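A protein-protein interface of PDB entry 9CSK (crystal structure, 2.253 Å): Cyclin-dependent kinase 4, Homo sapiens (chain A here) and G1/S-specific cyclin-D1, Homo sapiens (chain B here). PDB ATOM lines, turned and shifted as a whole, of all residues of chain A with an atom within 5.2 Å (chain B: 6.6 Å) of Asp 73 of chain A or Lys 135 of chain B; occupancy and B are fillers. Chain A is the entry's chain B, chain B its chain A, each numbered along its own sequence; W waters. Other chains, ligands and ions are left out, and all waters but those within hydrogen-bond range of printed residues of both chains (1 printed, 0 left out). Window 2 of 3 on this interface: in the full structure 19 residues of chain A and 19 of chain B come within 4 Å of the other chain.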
ATOM      1  N   SER A   4     -28.332 -15.990  27.966  1.00  0.00           N
ATOM      2  CA  SER A   4     -28.139 -15.180  29.177  1.00  0.00           C
ATOM      3  C   SER A   4     -26.650 -14.784  29.364  1.00  0.00           C
ATOM      4  O   SER A   4     -25.794 -15.293  28.636  1.00  0.00           O
ATOM      5  CB  SER A   4     -28.658 -15.923  30.412  1.00  0.00           C
ATOM      6  OG  SER A   4     -29.889 -16.596  30.186  1.00  0.00           O
ATOM      7  N   TYR A   6     -24.441 -15.156  32.179  1.00  0.00           N
ATOM      8  CA  TYR A   6     -24.150 -15.862  33.424  1.00  0.00           C
ATOM      9  C   TYR A   6     -22.939 -15.272  34.108  1.00  0.00           C
ATOM     10  O   TYR A   6     -21.882 -15.135  33.489  1.00  0.00           O
ATOM     11  CB  TYR A   6     -23.939 -17.375  33.165  1.00  0.00           C
ATOM     12  CG  TYR A   6     -24.895 -17.964  32.150  1.00  0.00           C
ATOM     13  CD1 TYR A   6     -24.608 -17.928  30.790  1.00  0.00           C
ATOM     14  CD2 TYR A   6     -26.118 -18.488  32.541  1.00  0.00           C
ATOM     15  CE1 TYR A   6     -25.502 -18.420  29.849  1.00  0.00           C
ATOM     16  CE2 TYR A   6     -27.012 -18.999  31.611  1.00  0.00           C
ATOM     17  CZ  TYR A   6     -26.703 -18.959  30.264  1.00  0.00           C
ATOM     18  OH  TYR A   6     -27.597 -19.442  29.341  1.00  0.00           O
ATOM     19  N   ARG A  58     -27.418 -30.575  21.222  1.00  0.00           N
ATOM     20  CA  ARG A  58     -28.609 -29.711  21.458  1.00  0.00           C
ATOM     21  C   ARG A  58     -29.878 -30.493  21.104  1.00  0.00           C
ATOM     22  O   ARG A  58     -30.878 -30.353  21.821  1.00  0.00           O
ATOM     23  CB  ARG A  58     -28.484 -28.413  20.655  1.00  0.00           C
ATOM     24  CG  ARG A  58     -27.400 -27.478  21.166  1.00  0.00           C
ATOM     25  CD  ARG A  58     -27.784 -26.830  22.478  1.00  0.00           C
ATOM     26  NE  ARG A  58     -28.489 -25.578  22.279  1.00  0.00           N
ATOM     27  CZ  ARG A  58     -29.300 -25.024  23.166  1.00  0.00           C
ATOM     28  NH1 ARG A  58     -29.526 -25.624  24.320  1.00  0.00           N
ATOM     29  NH2 ARG A  58     -29.891 -23.878  22.894  1.00  0.00           N
ATOM     30  N   LEU A  71     -27.537 -29.464  28.172  1.00  0.00           N
ATOM     31  CA  LEU A  71     -26.831 -28.369  27.530  1.00  0.00           C
ATOM     32  C   LEU A  71     -27.878 -27.325  27.217  1.00  0.00           C
ATOM     33  O   LEU A  71     -28.645 -27.493  26.273  1.00  0.00           O
ATOM     34  CB  LEU A  71     -26.207 -28.878  26.210  1.00  0.00           C
ATOM     35  CG  LEU A  71     -25.430 -27.868  25.386  1.00  0.00           C
ATOM     36  CD1 LEU A  71     -24.324 -27.220  26.199  1.00  0.00           C
ATOM     37  CD2 LEU A  71     -24.858 -28.512  24.154  1.00  0.00           C
ATOM     38  N   MET A  72     -27.932 -26.268  28.028  1.00  0.00           N
ATOM     39  CA  MET A  72     -28.998 -25.244  27.875  1.00  0.00           C
ATOM     40  C   MET A  72     -28.552 -24.046  27.030  1.00  0.00           C
ATOM     41  O   MET A  72     -29.439 -23.341  26.533  1.00  0.00           O
ATOM     42  CB  MET A  72     -29.481 -24.762  29.243  1.00  0.00           C
ATOM     43  CG  MET A  72     -29.972 -25.896  30.111  1.00  0.00           C
ATOM     44  SD  MET A  72     -30.281 -25.360  31.794  1.00  0.00           S
ATOM     45  CE  MET A  72     -28.776 -24.444  32.114  1.00  0.00           C
ATOM     46  N   ASP A  73     -27.249 -23.777  26.929  1.00  0.00           N
ATOM     47  CA  ASP A  73     -26.824 -22.617  26.105  1.00  0.00           C
ATOM     48  C   ASP A  73     -25.445 -22.869  25.488  1.00  0.00           C
ATOM     49  O   ASP A  73     -24.642 -23.574  26.110  1.00  0.00           O
ATOM     50  CB  ASP A  73     -26.889 -21.319  26.912  1.00  0.00           C
ATOM     51  CG  ASP A  73     -27.072 -20.084  26.054  1.00  0.00           C
ATOM     52  OD1 ASP A  73     -27.223 -20.244  24.833  1.00  0.00           O
ATOM     53  OD2 ASP A  73     -27.059 -18.977  26.617  1.00  0.00           O
ATOM     54  N   VAL A  74     -25.224 -22.364  24.271  1.00  0.00           N
ATOM     55  CA  VAL A  74     -23.905 -22.468  23.577  1.00  0.00           C
ATOM     56  C   VAL A  74     -23.590 -21.098  22.968  1.00  0.00           C
ATOM     57  O   VAL A  74     -24.498 -20.511  22.359  1.00  0.00           O
ATOM     58  CB  VAL A  74     -23.891 -23.555  22.485  1.00  0.00           C
ATOM     59  CG1 VAL A  74     -22.502 -23.707  21.890  1.00  0.00           C
ATOM     60  CG2 VAL A  74     -24.405 -24.898  22.978  1.00  0.00           C
ATOM     61  N   CYS A  75     -22.362 -20.603  23.126  1.00  0.00           N
ATOM     62  CA  CYS A  75     -22.013 -19.302  22.500  1.00  0.00           C
ATOM     63  C   CYS A  75     -20.561 -19.303  22.010  1.00  0.00           C
ATOM     64  O   CYS A  75     -19.685 -19.760  22.758  1.00  0.00           O
ATOM     65  CB  CYS A  75     -22.205 -18.154  23.481  1.00  0.00           C
ATOM     66  SG  CYS A  75     -22.042 -16.524  22.706  1.00  0.00           S
ATOM     67  N   THR A  87     -18.351 -21.573  24.204  1.00  0.00           N
ATOM     68  CA  THR A  87     -18.707 -21.763  25.632  1.00  0.00           C
ATOM     69  C   THR A  87     -19.988 -22.593  25.706  1.00  0.00           C
ATOM     70  O   THR A  87     -20.984 -22.189  25.089  1.00  0.00           O
ATOM     71  CB  THR A  87     -18.900 -20.416  26.332  1.00  0.00           C
ATOM     72  OG1 THR A  87     -17.601 -19.869  26.549  1.00  0.00           O
ATOM     73  CG2 THR A  87     -19.620 -20.542  27.655  1.00  0.00           C
ATOM     74  N   LEU A  88     -19.949 -23.696  26.456  1.00  0.00           N
ATOM     75  CA  LEU A  88     -21.125 -24.591  26.595  1.00  0.00           C
ATOM     76  C   LEU A  88     -21.717 -24.392  27.990  1.00  0.00           C
ATOM     77  O   LEU A  88     -20.964 -24.491  28.964  1.00  0.00           O
ATOM     78  CB  LEU A  88     -20.660 -26.037  26.399  1.00  0.00           C
ATOM     79  CG  LEU A  88     -19.952 -26.316  25.076  1.00  0.00           C
ATOM     80  CD1 LEU A  88     -18.954 -27.452  25.218  1.00  0.00           C
ATOM     81  CD2 LEU A  88     -20.954 -26.615  23.978  1.00  0.00           C
ATOM     82  N   VAL A  89     -23.023 -24.122  28.066  1.00  0.00           N
ATOM     83  CA  VAL A  89     -23.705 -23.908  29.376  1.00  0.00           C
ATOM     84  C   VAL A  89     -24.546 -25.146  29.700  1.00  0.00           C
ATOM     85  O   VAL A  89     -25.447 -25.469  28.912  1.00  0.00           O
ATOM     86  CB  VAL A  89     -24.559 -22.626  29.367  1.00  0.00           C
ATOM     87  CG1 VAL A  89     -25.141 -22.327  30.738  1.00  0.00           C
ATOM     88  CG2 VAL A  89     -23.770 -21.435  28.850  1.00  0.00           C
ATOM     89  N   ARG B  73     -36.073 -17.473  11.978  1.00  0.00           N
ATOM     90  CA  ARG B  73     -35.705 -17.419  13.417  1.00  0.00           C
ATOM     91  C   ARG B  73     -34.747 -16.255  13.682  1.00  0.00           C
ATOM     92  O   ARG B  73     -34.939 -15.565  14.692  1.00  0.00           O
ATOM     93  CB  ARG B  73     -35.095 -18.755  13.846  1.00  0.00           C
ATOM     94  CG  ARG B  73     -36.131 -19.845  14.070  1.00  0.00           C
ATOM     95  CD  ARG B  73     -35.531 -21.232  14.056  1.00  0.00           C
ATOM     96  NE  ARG B  73     -34.509 -21.448  15.064  1.00  0.00           N
ATOM     97  CZ  ARG B  73     -33.671 -22.472  15.064  1.00  0.00           C
ATOM     98  NH1 ARG B  73     -33.731 -23.372  14.101  1.00  0.00           N
ATOM     99  NH2 ARG B  73     -32.772 -22.592  16.021  1.00  0.00           N
ATOM    100  N   LEU B 130     -25.311 -15.792  13.249  1.00  0.00           N
ATOM    101  CA  LEU B 130     -26.439 -16.698  13.048  1.00  0.00           C
ATOM    102  C   LEU B 130     -26.423 -17.852  14.069  1.00  0.00           C
ATOM    103  O   LEU B 130     -27.379 -17.999  14.820  1.00  0.00           O
ATOM    104  CB  LEU B 130     -26.472 -17.225  11.599  1.00  0.00           C
ATOM    105  CG  LEU B 130     -27.570 -18.252  11.326  1.00  0.00           C
ATOM    106  CD1 LEU B 130     -28.929 -17.630  11.442  1.00  0.00           C
ATOM    107  CD2 LEU B 130     -27.376 -18.931   9.999  1.00  0.00           C
ATOM    108  N   VAL B 131     -25.327 -18.634  14.119  1.00  0.00           N
ATOM    109  CA  VAL B 131     -25.208 -19.772  15.026  1.00  0.00           C
ATOM    110  C   VAL B 131     -25.414 -19.347  16.501  1.00  0.00           C
ATOM    111  O   VAL B 131     -26.131 -20.019  17.226  1.00  0.00           O
ATOM    112  CB  VAL B 131     -23.884 -20.554  14.772  1.00  0.00           C
ATOM    113  CG1 VAL B 131     -23.612 -21.539  15.880  1.00  0.00           C
ATOM    114  CG2 VAL B 131     -23.941 -21.288  13.432  1.00  0.00           C
ATOM    115  N   ASN B 132     -24.856 -18.193  16.914  1.00  0.00           N
ATOM    116  CA  ASN B 132     -25.043 -17.676  18.277  1.00  0.00           C
ATOM    117  C   ASN B 132     -26.476 -17.235  18.558  1.00  0.00           C
ATOM    118  O   ASN B 132     -27.018 -17.643  19.572  1.00  0.00           O
ATOM    119  CB  ASN B 132     -24.066 -16.541  18.575  1.00  0.00           C
ATOM    120  CG  ASN B 132     -22.650 -17.021  18.771  1.00  0.00           C
ATOM    121  OD1 ASN B 132     -22.397 -18.208  19.007  1.00  0.00           O
ATOM    122  ND2 ASN B 132     -21.693 -16.115  18.703  1.00  0.00           N
ATOM    123  N   LYS B 133     -27.116 -16.460  17.664  1.00  0.00           N
ATOM    124  CA  LYS B 133     -28.510 -16.052  17.869  1.00  0.00           C
ATOM    125  C   LYS B 133     -29.438 -17.251  17.938  1.00  0.00           C
ATOM    126  O   LYS B 133     -30.429 -17.202  18.658  1.00  0.00           O
ATOM    127  CB  LYS B 133     -28.991 -15.071  16.787  1.00  0.00           C
ATOM    128  CG  LYS B 133     -28.629 -13.620  17.098  1.00  0.00           C
ATOM    129  CD  LYS B 133     -29.561 -12.989  18.126  1.00  0.00           C
ATOM    130  CE  LYS B 133     -28.885 -11.795  18.782  1.00  0.00           C
ATOM    131  NZ  LYS B 133     -29.857 -10.850  19.415  1.00  0.00           N
ATOM    132  N   LEU B 134     -29.149 -18.317  17.190  1.00  0.00           N
ATOM    133  CA  LEU B 134     -29.962 -19.530  17.244  1.00  0.00           C
ATOM    134  C   LEU B 134     -29.599 -20.456  18.414  1.00  0.00           C
ATOM    135  O   LEU B 134     -30.201 -21.517  18.547  1.00  0.00           O
ATOM    136  CB  LEU B 134     -29.874 -20.317  15.930  1.00  0.00           C
ATOM    137  CG  LEU B 134     -30.261 -19.595  14.651  1.00  0.00           C
ATOM    138  CD1 LEU B 134     -30.164 -20.522  13.480  1.00  0.00           C
ATOM    139  CD2 LEU B 134     -31.647 -19.023  14.738  1.00  0.00           C
ATOM    140  N   LYS B 135     -28.622 -20.062  19.246  1.00  0.00           N
ATOM    141  CA  LYS B 135     -28.084 -20.786  20.396  1.00  0.00           C
ATOM    142  C   LYS B 135     -27.664 -22.212  20.030  1.00  0.00           C
ATOM    143  O   LYS B 135     -27.828 -23.144  20.824  1.00  0.00           O
ATOM    144  CB  LYS B 135     -29.044 -20.722  21.591  1.00  0.00           C
ATOM    145  CG  LYS B 135     -29.177 -19.295  22.124  1.00  0.00           C
ATOM    146  CD  LYS B 135     -30.290 -19.155  23.121  1.00  0.00           C
ATOM    147  CE  LYS B 135     -30.039 -18.021  24.080  1.00  0.00           C
ATOM    148  NZ  LYS B 135     -30.886 -18.171  25.302  1.00  0.00           N
ATOM    149  N   TRP B 136     -27.088 -22.348  18.816  1.00  0.00           N
ATOM    150  CA  TRP B 136     -26.625 -23.578  18.180  1.00  0.00           C
ATOM    151  C   TRP B 136     -27.716 -24.639  18.089  1.00  0.00           C
ATOM    152  O   TRP B 136     -27.407 -25.827  18.141  1.00  0.00           O
ATOM    153  CB  TRP B 136     -25.349 -24.119  18.809  1.00  0.00           C
ATOM    154  CG  TRP B 136     -24.166 -23.204  18.669  1.00  0.00           C
ATOM    155  CD1 TRP B 136     -24.041 -21.935  19.163  1.00  0.00           C
ATOM    156  CD2 TRP B 136     -22.898 -23.536  18.089  1.00  0.00           C
ATOM    157  NE1 TRP B 136     -22.787 -21.445  18.891  1.00  0.00           N
ATOM    158  CE2 TRP B 136     -22.056 -22.417  18.256  1.00  0.00           C
ATOM    159  CE3 TRP B 136     -22.383 -24.682  17.480  1.00  0.00           C
ATOM    160  CZ2 TRP B 136     -20.716 -22.422  17.849  1.00  0.00           C
ATOM    161  CZ3 TRP B 136     -21.055 -24.691  17.095  1.00  0.00           C
ATOM    162  CH2 TRP B 136     -20.240 -23.569  17.269  1.00  0.00           C
ATOM    163  N   ASN B 137     -28.984 -24.226  17.942  1.00  0.00           N
ATOM    164  CA  ASN B 137     -30.090 -25.161  17.746  1.00  0.00           C
ATOM    165  C   ASN B 137     -30.188 -25.309  16.231  1.00  0.00           C
ATOM    166  O   ASN B 137     -31.030 -24.685  15.585  1.00  0.00           O
ATOM    167  CB  ASN B 137     -31.398 -24.595  18.295  1.00  0.00           C
ATOM    168  CG  ASN B 137     -31.593 -24.819  19.761  1.00  0.00           C
ATOM    169  OD1 ASN B 137     -31.249 -25.876  20.290  1.00  0.00           O
ATOM    170  ND2 ASN B 137     -32.164 -23.826  20.444  1.00  0.00           N
ATOM    171  N   LEU B 138     -29.257 -26.063  15.654  1.00  0.00           N
ATOM    172  CA  LEU B 138     -29.137 -26.176  14.211  1.00  0.00           C
ATOM    173  C   LEU B 138     -29.769 -27.438  13.643  1.00  0.00           C
ATOM    174  O   LEU B 138     -30.162 -27.456  12.475  1.00  0.00           O
ATOM    175  CB  LEU B 138     -27.668 -26.051  13.800  1.00  0.00           C
ATOM    176  CG  LEU B 138     -26.872 -24.879  14.403  1.00  0.00           C
ATOM    177  CD1 LEU B 138     -25.381 -24.966  14.014  1.00  0.00           C
ATOM    178  CD2 LEU B 138     -27.470 -23.550  14.024  1.00  0.00           C
HETATM  179  O   HOH W   1     -25.723 -17.869  21.903  1.00  0.00           O
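The backbone carbonyl oxygen (O) of Lys 135 of chain B lies within hydrogen-bond range of the guanidinium group (NE) of Arg 58 of chain A (2.9 Å).
The guanidinium group (NH2) of Arg 58 of chain A sits close to the side-chain amide nitrogen (ND2) of Asn 137 of chain B (3.3 Å).
The backbone NH (N) of Val 89 of chain A sits at hydrogen-bond distance from the backbone carbonyl oxygen (O) of Asp 73 of chain A (2.6 Å).
The side-chain hydroxyl (OH) of Tyr 6 of chain A is in hydrogen-bond range of the side-chain carboxylate (OD2) of Asp 73 of chain A (2.8 Å).
The indole nitrogen (NE1) of Trp 136 of chain B sits at hydrogen-bond distance from the side-chain amide oxygen (OD1) of Asn 132 of chain B, 3.3 Å away.
The guanidinium group (NH1) of Arg 58 of chain A is in hydrogen-bond range of the backbone carbonyl oxygen (O) of Leu 71 of chain A (2.8 Å).
O of Val 131 of chain B is in hydrogen-bond range of N of Trp 136 of chain B (3.0 Å).
The guanidinium group (NH2) of Arg 73 of chain B is in hydrogen-bond range of the backbone carbonyl oxygen (O) of Asn 137 of chain B, 2.8 Å away.
O of Trp 136 of chain B touches CG of Arg 58 of chain A (3.4 Å).
Asp 73 of chain A touches Lys 135 of chain B (OD1 to CG, 3.5 Å).
O of Val 74 of chain A touches CD1 of Trp 136 of chain B (3.5 Å).
Asn 132 of chain B touches Cys 75 of chain A.
Asp 73 of chain A touches just one residue of chain B: Lys 135.
Val 131 of chain B touches none of the printed residues of chain A.
Of the printed residues of chain A, Asn 132 of chain B touches Cys 75 (3.7 Å).
Lys 135 of chain B touches two residues of chain A.
Printed residues of chain A within 4 Å of Trp 136 of chain B: Arg 58 and Val 74.
Of the printed residues of chain A, Asn 137 of chain B touches Arg 58 (3.3 Å).
Of the 10 printed residues of chain B, 4 touch a printed residue of chain A.
Hydrophobic or aromatic side chains of chain A within 4 Å of the printed part of chain B: Val 74.
Along chain A the printed residues that touch a printed residue of chain B span positions 58 to 75.
Water W1 lies within hydrogen-bond range of the backbone carbonyl oxygen of Asn 132 of chain B (2.7 Å) and the backbone carbonyl oxygen of Val 74 of chain A (2.9 Å).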
